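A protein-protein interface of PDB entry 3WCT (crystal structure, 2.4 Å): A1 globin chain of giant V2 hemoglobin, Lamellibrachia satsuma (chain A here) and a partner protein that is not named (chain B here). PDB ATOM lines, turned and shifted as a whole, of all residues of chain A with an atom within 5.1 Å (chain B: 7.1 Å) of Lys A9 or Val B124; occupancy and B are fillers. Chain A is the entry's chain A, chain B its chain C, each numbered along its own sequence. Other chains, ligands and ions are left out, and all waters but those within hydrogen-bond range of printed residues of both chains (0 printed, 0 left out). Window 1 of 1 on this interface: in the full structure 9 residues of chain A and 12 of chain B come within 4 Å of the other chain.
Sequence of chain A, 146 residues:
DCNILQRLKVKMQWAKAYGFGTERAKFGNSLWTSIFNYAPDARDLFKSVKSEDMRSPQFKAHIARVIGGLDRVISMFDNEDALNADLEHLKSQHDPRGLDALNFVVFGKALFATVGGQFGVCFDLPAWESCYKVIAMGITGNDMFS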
ATOM      1  N   LEU A   5       8.507  34.723 -13.976  1.00  0.00           N
ATOM      2  CA  LEU A   5       8.228  33.297 -14.084  1.00  0.00           C
ATOM      3  C   LEU A   5       7.038  32.892 -13.195  1.00  0.00           C
ATOM      4  O   LEU A   5       6.105  32.230 -13.646  1.00  0.00           O
ATOM      5  CB  LEU A   5       9.482  32.496 -13.715  1.00  0.00           C
ATOM      6  CG  LEU A   5      10.743  32.821 -14.541  1.00  0.00           C
ATOM      7  CD1 LEU A   5      11.836  31.801 -14.230  1.00  0.00           C
ATOM      8  CD2 LEU A   5      10.434  32.790 -16.031  1.00  0.00           C
ATOM      9  N   GLN A   6       7.075  33.309 -11.937  1.00  0.00           N
ATOM     10  CA  GLN A   6       6.018  33.007 -10.991  1.00  0.00           C
ATOM     11  C   GLN A   6       4.696  33.680 -11.346  1.00  0.00           C
ATOM     12  O   GLN A   6       3.624  33.203 -10.956  1.00  0.00           O
ATOM     13  CB  GLN A   6       6.453  33.425  -9.593  1.00  0.00           C
ATOM     14  CG  GLN A   6       7.748  32.784  -9.173  1.00  0.00           C
ATOM     15  CD  GLN A   6       8.092  33.104  -7.750  1.00  0.00           C
ATOM     16  OE1 GLN A   6       7.937  34.245  -7.311  1.00  0.00           O
ATOM     17  NE2 GLN A   6       8.570  32.106  -7.012  1.00  0.00           N
ATOM     18  N   ARG A   7       4.770  34.787 -12.079  1.00  0.00           N
ATOM     19  CA  ARG A   7       3.574  35.502 -12.493  1.00  0.00           C
ATOM     20  C   ARG A   7       2.868  34.717 -13.589  1.00  0.00           C
ATOM     21  O   ARG A   7       1.644  34.707 -13.665  1.00  0.00           O
ATOM     22  CB  ARG A   7       3.934  36.894 -13.019  1.00  0.00           C
ATOM     23  CG  ARG A   7       4.560  37.770 -11.974  1.00  0.00           C
ATOM     24  CD  ARG A   7       4.545  39.240 -12.342  1.00  0.00           C
ATOM     25  NE  ARG A   7       5.044  40.029 -11.220  1.00  0.00           N
ATOM     26  CZ  ARG A   7       4.838  41.332 -11.062  1.00  0.00           C
ATOM     27  NH1 ARG A   7       4.142  42.018 -11.961  1.00  0.00           N
ATOM     28  NH2 ARG A   7       5.305  41.941  -9.981  1.00  0.00           N
ATOM     29  N   LEU A   8       3.657  34.070 -14.442  1.00  0.00           N
ATOM     30  CA  LEU A   8       3.117  33.281 -15.541  1.00  0.00           C
ATOM     31  C   LEU A   8       2.563  31.987 -14.970  1.00  0.00           C
ATOM     32  O   LEU A   8       1.537  31.490 -15.421  1.00  0.00           O
ATOM     33  CB  LEU A   8       4.217  32.972 -16.561  1.00  0.00           C
ATOM     34  CG  LEU A   8       4.829  34.165 -17.307  1.00  0.00           C
ATOM     35  CD1 LEU A   8       6.036  33.687 -18.105  1.00  0.00           C
ATOM     36  CD2 LEU A   8       3.791  34.814 -18.225  1.00  0.00           C
ATOM     37  N   LYS A   9       3.266  31.456 -13.972  1.00  0.00           N
ATOM     38  CA  LYS A   9       2.882  30.226 -13.287  1.00  0.00           C
ATOM     39  C   LYS A   9       1.518  30.449 -12.625  1.00  0.00           C
ATOM     40  O   LYS A   9       0.597  29.652 -12.789  1.00  0.00           O
ATOM     41  CB  LYS A   9       3.929  29.890 -12.227  1.00  0.00           C
ATOM     42  CG  LYS A   9       3.686  28.598 -11.479  1.00  0.00           C
ATOM     43  CD  LYS A   9       3.746  27.403 -12.416  1.00  0.00           C
ATOM     44  CE  LYS A   9       4.172  26.151 -11.679  1.00  0.00           C
ATOM     45  NZ  LYS A   9       5.478  26.348 -11.008  1.00  0.00           N
ATOM     46  N   VAL A  10       1.409  31.549 -11.887  1.00  0.00           N
ATOM     47  CA  VAL A  10       0.172  31.917 -11.210  1.00  0.00           C
ATOM     48  C   VAL A  10      -0.968  32.143 -12.205  1.00  0.00           C
ATOM     49  O   VAL A  10      -2.105  31.785 -11.918  1.00  0.00           O
ATOM     50  CB  VAL A  10       0.392  33.176 -10.330  1.00  0.00           C
ATOM     51  CG1 VAL A  10      -0.925  33.725  -9.819  1.00  0.00           C
ATOM     52  CG2 VAL A  10       1.286  32.815  -9.163  1.00  0.00           C
ATOM     53  N   LYS A  11      -0.678  32.723 -13.368  1.00  0.00           N
ATOM     54  CA  LYS A  11      -1.725  32.920 -14.372  1.00  0.00           C
ATOM     55  C   LYS A  11      -2.212  31.575 -14.921  1.00  0.00           C
ATOM     56  O   LYS A  11      -3.396  31.402 -15.189  1.00  0.00           O
ATOM     57  CB  LYS A  11      -1.231  33.782 -15.533  1.00  0.00           C
ATOM     58  CG  LYS A  11      -1.150  35.255 -15.216  1.00  0.00           C
ATOM     59  CD  LYS A  11      -0.702  36.056 -16.430  1.00  0.00           C
ATOM     60  CE  LYS A  11      -1.738  36.012 -17.535  1.00  0.00           C
ATOM     61  NZ  LYS A  11      -1.268  36.779 -18.719  1.00  0.00           N
ATOM     62  N   MET A  12      -1.288  30.638 -15.097  1.00  0.00           N
ATOM     63  CA  MET A  12      -1.618  29.306 -15.594  1.00  0.00           C
ATOM     64  C   MET A  12      -2.568  28.634 -14.622  1.00  0.00           C
ATOM     65  O   MET A  12      -3.685  28.241 -14.979  1.00  0.00           O
ATOM     66  CB  MET A  12      -0.372  28.433 -15.676  1.00  0.00           C
ATOM     67  CG  MET A  12       0.678  28.945 -16.603  1.00  0.00           C
ATOM     68  SD  MET A  12       0.183  28.706 -18.303  1.00  0.00           S
ATOM     69  CE  MET A  12       1.796  28.489 -19.076  1.00  0.00           C
ATOM     70  N   GLN A  13      -2.103  28.495 -13.385  1.00  0.00           N
ATOM     71  CA  GLN A  13      -2.891  27.843 -12.369  1.00  0.00           C
ATOM     72  C   GLN A  13      -4.210  28.556 -12.096  1.00  0.00           C
ATOM     73  O   GLN A  13      -5.245  27.908 -11.963  1.00  0.00           O
ATOM     74  CB  GLN A  13      -2.035  27.641 -11.117  1.00  0.00           C
ATOM     75  CG  GLN A  13      -0.736  26.872 -11.456  1.00  0.00           C
ATOM     76  CD  GLN A  13       0.042  26.389 -10.242  1.00  0.00           C
ATOM     77  OE1 GLN A  13      -0.127  26.888  -9.122  1.00  0.00           O
ATOM     78  NE2 GLN A  13       0.920  25.423 -10.464  1.00  0.00           N
ATOM     79  N   TRP A  14      -4.205  29.882 -12.047  1.00  0.00           N
ATOM     80  CA  TRP A  14      -5.461  30.591 -11.832  1.00  0.00           C
ATOM     81  C   TRP A  14      -6.456  30.250 -12.950  1.00  0.00           C
ATOM     82  O   TRP A  14      -7.639  30.031 -12.688  1.00  0.00           O
ATOM     83  CB  TRP A  14      -5.243  32.105 -11.803  1.00  0.00           C
ATOM     84  CG  TRP A  14      -6.502  32.875 -12.017  1.00  0.00           C
ATOM     85  CD1 TRP A  14      -6.951  33.392 -13.191  1.00  0.00           C
ATOM     86  CD2 TRP A  14      -7.513  33.156 -11.038  1.00  0.00           C
ATOM     87  NE1 TRP A  14      -8.179  33.980 -13.011  1.00  0.00           N
ATOM     88  CE2 TRP A  14      -8.548  33.852 -11.697  1.00  0.00           C
ATOM     89  CE3 TRP A  14      -7.642  32.890  -9.664  1.00  0.00           C
ATOM     90  CZ2 TRP A  14      -9.708  34.289 -11.031  1.00  0.00           C
ATOM     91  CZ3 TRP A  14      -8.789  33.321  -8.995  1.00  0.00           C
ATOM     92  CH2 TRP A  14      -9.812  34.020  -9.688  1.00  0.00           C
ATOM     93  N   CYS A 122       0.085  20.046  -8.009  1.00  0.00           N
ATOM     94  CA  CYS A 122       1.185  20.812  -8.591  1.00  0.00           C
ATOM     95  C   CYS A 122       1.025  22.304  -8.307  1.00  0.00           C
ATOM     96  O   CYS A 122       1.742  23.135  -8.855  1.00  0.00           O
ATOM     97  CB  CYS A 122       1.276  20.556 -10.096  1.00  0.00           C
ATOM     98  SG  CYS A 122       1.311  18.783 -10.514  1.00  0.00           S
ATOM     99  N   ASP A 124       1.514  25.756  -6.990  1.00  0.00           N
ATOM    100  CA  ASP A 124       2.795  26.340  -6.595  1.00  0.00           C
ATOM    101  C   ASP A 124       2.522  27.325  -5.459  1.00  0.00           C
ATOM    102  O   ASP A 124       2.270  28.501  -5.705  1.00  0.00           O
ATOM    103  CB  ASP A 124       3.434  27.068  -7.794  1.00  0.00           C
ATOM    104  CG  ASP A 124       4.933  27.328  -7.602  1.00  0.00           C
ATOM    105  OD1 ASP A 124       5.340  27.694  -6.481  1.00  0.00           O
ATOM    106  OD2 ASP A 124       5.698  27.172  -8.577  1.00  0.00           O
ATOM    107  N   ALA A 127       5.037  30.522  -5.091  1.00  0.00           N
ATOM    108  CA  ALA A 127       4.785  31.517  -6.126  1.00  0.00           C
ATOM    109  C   ALA A 127       3.507  32.285  -5.802  1.00  0.00           C
ATOM    110  O   ALA A 127       3.427  33.502  -6.001  1.00  0.00           O
ATOM    111  CB  ALA A 127       4.654  30.851  -7.480  1.00  0.00           C
ATOM    112  N   MET B  16       4.934  18.703 -20.055  1.00  0.00           N
ATOM    113  CA  MET B  16       5.570  19.779 -19.293  1.00  0.00           C
ATOM    114  C   MET B  16       5.678  21.033 -20.154  1.00  0.00           C
ATOM    115  O   MET B  16       5.454  22.151 -19.688  1.00  0.00           O
ATOM    116  CB  MET B  16       6.975  19.368 -18.844  1.00  0.00           C
ATOM    117  CG  MET B  16       7.028  18.233 -17.842  1.00  0.00           C
ATOM    118  SD  MET B  16       8.731  17.859 -17.334  1.00  0.00           S
ATOM    119  CE  MET B  16       9.024  16.316 -18.191  1.00  0.00           C
ATOM    120  N   ASN B  19       1.932  22.536 -21.921  1.00  0.00           N
ATOM    121  CA  ASN B  19       1.132  23.280 -20.959  1.00  0.00           C
ATOM    122  C   ASN B  19       1.641  24.703 -20.755  1.00  0.00           C
ATOM    123  O   ASN B  19       0.845  25.644 -20.701  1.00  0.00           O
ATOM    124  CB  ASN B  19       1.075  22.544 -19.612  1.00  0.00           C
ATOM    125  CG  ASN B  19      -0.057  21.525 -19.551  1.00  0.00           C
ATOM    126  OD1 ASN B  19      -0.043  20.506 -20.248  1.00  0.00           O
ATOM    127  ND2 ASN B  19      -1.052  21.806 -18.717  1.00  0.00           N
ATOM    128  N   VAL B  20       2.957  24.867 -20.654  1.00  0.00           N
ATOM    129  CA  VAL B  20       3.528  26.194 -20.449  1.00  0.00           C
ATOM    130  C   VAL B  20       3.596  26.998 -21.743  1.00  0.00           C
ATOM    131  O   VAL B  20       3.521  28.227 -21.736  1.00  0.00           O
ATOM    132  CB  VAL B  20       4.937  26.105 -19.867  1.00  0.00           C
ATOM    133  CG1 VAL B  20       5.343  27.456 -19.309  1.00  0.00           C
ATOM    134  CG2 VAL B  20       4.981  25.038 -18.792  1.00  0.00           C
ATOM    135  N   ARG B  28       4.836  34.245 -22.993  1.00  0.00           N
ATOM    136  CA  ARG B  28       5.338  33.121 -22.213  1.00  0.00           C
ATOM    137  C   ARG B  28       6.706  32.636 -22.710  1.00  0.00           C
ATOM    138  O   ARG B  28       7.674  32.624 -21.954  1.00  0.00           O
ATOM    139  CB  ARG B  28       4.315  31.977 -22.252  1.00  0.00           C
ATOM    140  CG  ARG B  28       4.090  31.279 -20.919  1.00  0.00           C
ATOM    141  CD  ARG B  28       2.604  31.270 -20.560  1.00  0.00           C
ATOM    142  NE  ARG B  28       1.790  30.636 -21.599  1.00  0.00           N
ATOM    143  CZ  ARG B  28       0.458  30.621 -21.620  1.00  0.00           C
ATOM    144  NH1 ARG B  28      -0.185  30.016 -22.615  1.00  0.00           N
ATOM    145  NH2 ARG B  28      -0.236  31.216 -20.655  1.00  0.00           N
ATOM    146  N   ALA B  31       9.540  35.109 -22.095  1.00  0.00           N
ATOM    147  CA  ALA B  31       9.873  35.160 -20.680  1.00  0.00           C
ATOM    148  C   ALA B  31      10.723  33.967 -20.247  1.00  0.00           C
ATOM    149  O   ALA B  31      11.647  34.121 -19.453  1.00  0.00           O
ATOM    150  CB  ALA B  31       8.597  35.219 -19.856  1.00  0.00           C
ATOM    151  N   ILE B  32      10.404  32.784 -20.770  1.00  0.00           N
ATOM    152  CA  ILE B  32      11.130  31.558 -20.440  1.00  0.00           C
ATOM    153  C   ILE B  32      12.564  31.544 -20.968  1.00  0.00           C
ATOM    154  O   ILE B  32      13.475  31.073 -20.281  1.00  0.00           O
ATOM    155  CB  ILE B  32      10.414  30.302 -21.006  1.00  0.00           C
ATOM    156  CG1 ILE B  32       9.054  30.115 -20.339  1.00  0.00           C
ATOM    157  CG2 ILE B  32      11.265  29.074 -20.776  1.00  0.00           C
ATOM    158  CD1 ILE B  32       8.331  28.876 -20.802  1.00  0.00           C
ATOM    159  N   ARG B 119      16.689  25.083 -13.777  1.00  0.00           N
ATOM    160  CA  ARG B 119      16.401  26.076 -12.745  1.00  0.00           C
ATOM    161  C   ARG B 119      15.215  26.967 -13.117  1.00  0.00           C
ATOM    162  O   ARG B 119      14.512  27.475 -12.243  1.00  0.00           O
ATOM    163  CB  ARG B 119      17.622  26.967 -12.501  1.00  0.00           C
ATOM    164  CG  ARG B 119      18.568  26.500 -11.391  1.00  0.00           C
ATOM    165  CD  ARG B 119      19.594  27.599 -11.093  1.00  0.00           C
ATOM    166  NE  ARG B 119      20.458  27.872 -12.238  1.00  0.00           N
ATOM    167  CZ  ARG B 119      21.554  27.175 -12.526  1.00  0.00           C
ATOM    168  NH1 ARG B 119      22.281  27.485 -13.594  1.00  0.00           N
ATOM    169  NH2 ARG B 119      21.933  26.181 -11.732  1.00  0.00           N
ATOM    170  N   VAL B 120      14.995  27.153 -14.415  1.00  0.00           N
ATOM    171  CA  VAL B 120      13.904  28.001 -14.895  1.00  0.00           C
ATOM    172  C   VAL B 120      12.528  27.314 -14.981  1.00  0.00           C
ATOM    173  O   VAL B 120      11.525  27.845 -14.497  1.00  0.00           O
ATOM    174  CB  VAL B 120      14.220  28.568 -16.296  1.00  0.00           C
ATOM    175  CG1 VAL B 120      13.093  29.472 -16.735  1.00  0.00           C
ATOM    176  CG2 VAL B 120      15.525  29.325 -16.280  1.00  0.00           C
ATOM    177  N   MET B 121      12.496  26.145 -15.612  1.00  0.00           N
ATOM    178  CA  MET B 121      11.269  25.385 -15.800  1.00  0.00           C
ATOM    179  C   MET B 121      10.424  25.178 -14.545  1.00  0.00           C
ATOM    180  O   MET B 121       9.247  25.524 -14.525  1.00  0.00           O
ATOM    181  CB  MET B 121      11.604  24.035 -16.438  1.00  0.00           C
ATOM    182  CG  MET B 121      12.244  24.165 -17.820  1.00  0.00           C
ATOM    183  SD  MET B 121      11.214  25.109 -18.976  1.00  0.00           S
ATOM    184  CE  MET B 121       9.817  23.993 -19.116  1.00  0.00           C
ATOM    185  N   PRO B 122      11.011  24.611 -13.482  1.00  0.00           N
ATOM    186  CA  PRO B 122      10.216  24.399 -12.269  1.00  0.00           C
ATOM    187  C   PRO B 122       9.477  25.643 -11.787  1.00  0.00           C
ATOM    188  O   PRO B 122       8.377  25.539 -11.249  1.00  0.00           O
ATOM    189  CB  PRO B 122      11.240  23.880 -11.256  1.00  0.00           C
ATOM    190  CG  PRO B 122      12.554  24.398 -11.776  1.00  0.00           C
ATOM    191  CD  PRO B 122      12.422  24.248 -13.265  1.00  0.00           C
ATOM    192  N   GLN B 123      10.069  26.813 -12.009  1.00  0.00           N
ATOM    193  CA  GLN B 123       9.473  28.082 -11.586  1.00  0.00           C
ATOM    194  C   GLN B 123       8.243  28.454 -12.401  1.00  0.00           C
ATOM    195  O   GLN B 123       7.344  29.141 -11.909  1.00  0.00           O
ATOM    196  CB  GLN B 123      10.469  29.230 -11.745  1.00  0.00           C
ATOM    197  CG  GLN B 123      11.662  29.224 -10.832  1.00  0.00           C
ATOM    198  CD  GLN B 123      12.639  30.313 -11.223  1.00  0.00           C
ATOM    199  OE1 GLN B 123      12.286  31.486 -11.278  1.00  0.00           O
ATOM    200  NE2 GLN B 123      13.865  29.927 -11.516  1.00  0.00           N
ATOM    201  N   VAL B 124       8.212  28.015 -13.652  1.00  0.00           N
ATOM    202  CA  VAL B 124       7.107  28.364 -14.531  1.00  0.00           C
ATOM    203  C   VAL B 124       6.212  27.189 -14.933  1.00  0.00           C
ATOM    204  O   VAL B 124       5.028  27.379 -15.225  1.00  0.00           O
ATOM    205  CB  VAL B 124       7.663  29.096 -15.793  1.00  0.00           C
ATOM    206  CG1 VAL B 124       8.691  28.211 -16.494  1.00  0.00           C
ATOM    207  CG2 VAL B 124       6.531  29.493 -16.731  1.00  0.00           C
ATOM    208  N   ALA B 125       6.765  25.980 -14.931  1.00  0.00           N
ATOM    209  CA  ALA B 125       6.003  24.791 -15.306  1.00  0.00           C
ATOM    210  C   ALA B 125       5.428  24.074 -14.090  1.00  0.00           C
ATOM    211  O   ALA B 125       6.104  23.908 -13.076  1.00  0.00           O
ATOM    212  CB  ALA B 125       6.887  23.833 -16.097  1.00  0.00           C
ATOM    213  N   SER B 126       4.171  23.659 -14.202  1.00  0.00           N
ATOM    214  CA  SER B 126       3.489  22.941 -13.131  1.00  0.00           C
ATOM    215  C   SER B 126       3.722  21.457 -13.362  1.00  0.00           C
ATOM    216  O   SER B 126       3.760  21.007 -14.503  1.00  0.00           O
ATOM    217  CB  SER B 126       1.980  23.209 -13.168  1.00  0.00           C
ATOM    218  OG  SER B 126       1.673  24.557 -12.887  1.00  0.00           O
ATOM    219  N   CYS B 127       3.867  20.699 -12.281  1.00  0.00           N
ATOM    220  CA  CYS B 127       4.089  19.263 -12.394  1.00  0.00           C
ATOM    221  C   CYS B 127       5.382  18.965 -13.170  1.00  0.00           C
ATOM    222  O   CYS B 127       5.401  18.056 -14.009  1.00  0.00           O
ATOM    223  CB  CYS B 127       2.930  18.594 -13.143  1.00  0.00           C
ATOM    224  SG  CYS B 127       1.211  18.773 -12.545  1.00  0.00           S
ATOM    225  N   PHE B 128       6.448  19.723 -12.901  1.00  0.00           N
ATOM    226  CA  PHE B 128       7.729  19.530 -13.592  1.00  0.00           C
ATOM    227  C   PHE B 128       8.453  18.268 -13.128  1.00  0.00           C
ATOM    228  O   PHE B 128       8.631  18.047 -11.930  1.00  0.00           O
ATOM    229  CB  PHE B 128       8.644  20.746 -13.390  1.00  0.00           C
ATOM    230  CG  PHE B 128       9.951  20.659 -14.148  1.00  0.00           C
ATOM    231  CD1 PHE B 128       9.967  20.603 -15.541  1.00  0.00           C
ATOM    232  CD2 PHE B 128      11.159  20.614 -13.473  1.00  0.00           C
ATOM    233  CE1 PHE B 128      11.172  20.502 -16.249  1.00  0.00           C
ATOM    234  CE2 PHE B 128      12.360  20.515 -14.167  1.00  0.00           C
ATOM    235  CZ  PHE B 128      12.366  20.458 -15.559  1.00  0.00           C
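SG of Cys A122 forms a disulfide with SG of Cys B127 (2.0 Å). O of Ala B125 sits at hydrogen-bond distance from NZ of Lys A9 (3.3 Å). NE2 of Gln A13 sits at hydrogen-bond distance from OG of Ser B126, at 2.7 Å. NZ of Lys A9 is in hydrogen-bond range of O of Pro B122 (3.0 Å). O of Gln B123 is in hydrogen-bond range of NZ of Lys A9 (3.5 Å). The side-chain sulfur (SD) of Met A12 lies within hydrogen-bond range of the guanidinium group (NH2) of Arg B28, at 3.5 Å.
NZ of Lys A9 lies within salt-bridge range of OD2 of Asp A124 (2.6 Å). O of Arg B119 sits at hydrogen-bond distance from NE2 of Gln B123 (2.6 Å). The backbone carbonyl oxygen (O) of Val B20 lies within hydrogen-bond range of the guanidinium group (NE) of Arg B28 (3.0 Å). NE2 of Gln A13 sits at hydrogen-bond distance from O of Cys A122 (2.9 Å). The side-chain amide oxygen (OE1) of Gln A13 lies within hydrogen-bond range of the backbone NH (N) of Asp A124, 2.9 Å away.
Among the printed residues, pairs that only touch across the chains: Leu A5 with Gln B123, Lys A9 with Val B124, Met A12 with Val B20, Lys A9 with Ser B126, Met A12 with Asn B19, Leu A8 with Ala B31, Leu A5 with Val B120 and Leu A5 with Ala B31.
Lys A11 touches none of the printed residues of chain B. Of the printed residues of chain A, Arg B28 touches Met A12 (3.3 Å). Of chain A, only Lys A9 comes within 4 Å of Val B124. Printed residues of chain A within 4 Å of Cys B127: Cys A122 (2.0 Å).
Of the 13 printed residues of chain A, 6 touch a printed residue of chain B. Along chain A the printed residues that touch a printed residue of chain B span positions 5 to 122. Of the 16 printed residues of chain B, 11 touch a printed residue of chain A. Printed residues of chain B that touch a printed residue of chain A: Asn B19, Val B20, Arg B28, Ala B31, Val B120, Pro B122, Gln B123, Val B124, Ala B125, Ser B126 and Cys B127. Hydrophobic or aromatic side chains of chain B that line the printed part of chain A: Val B20, Ala B31 and Val B120.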
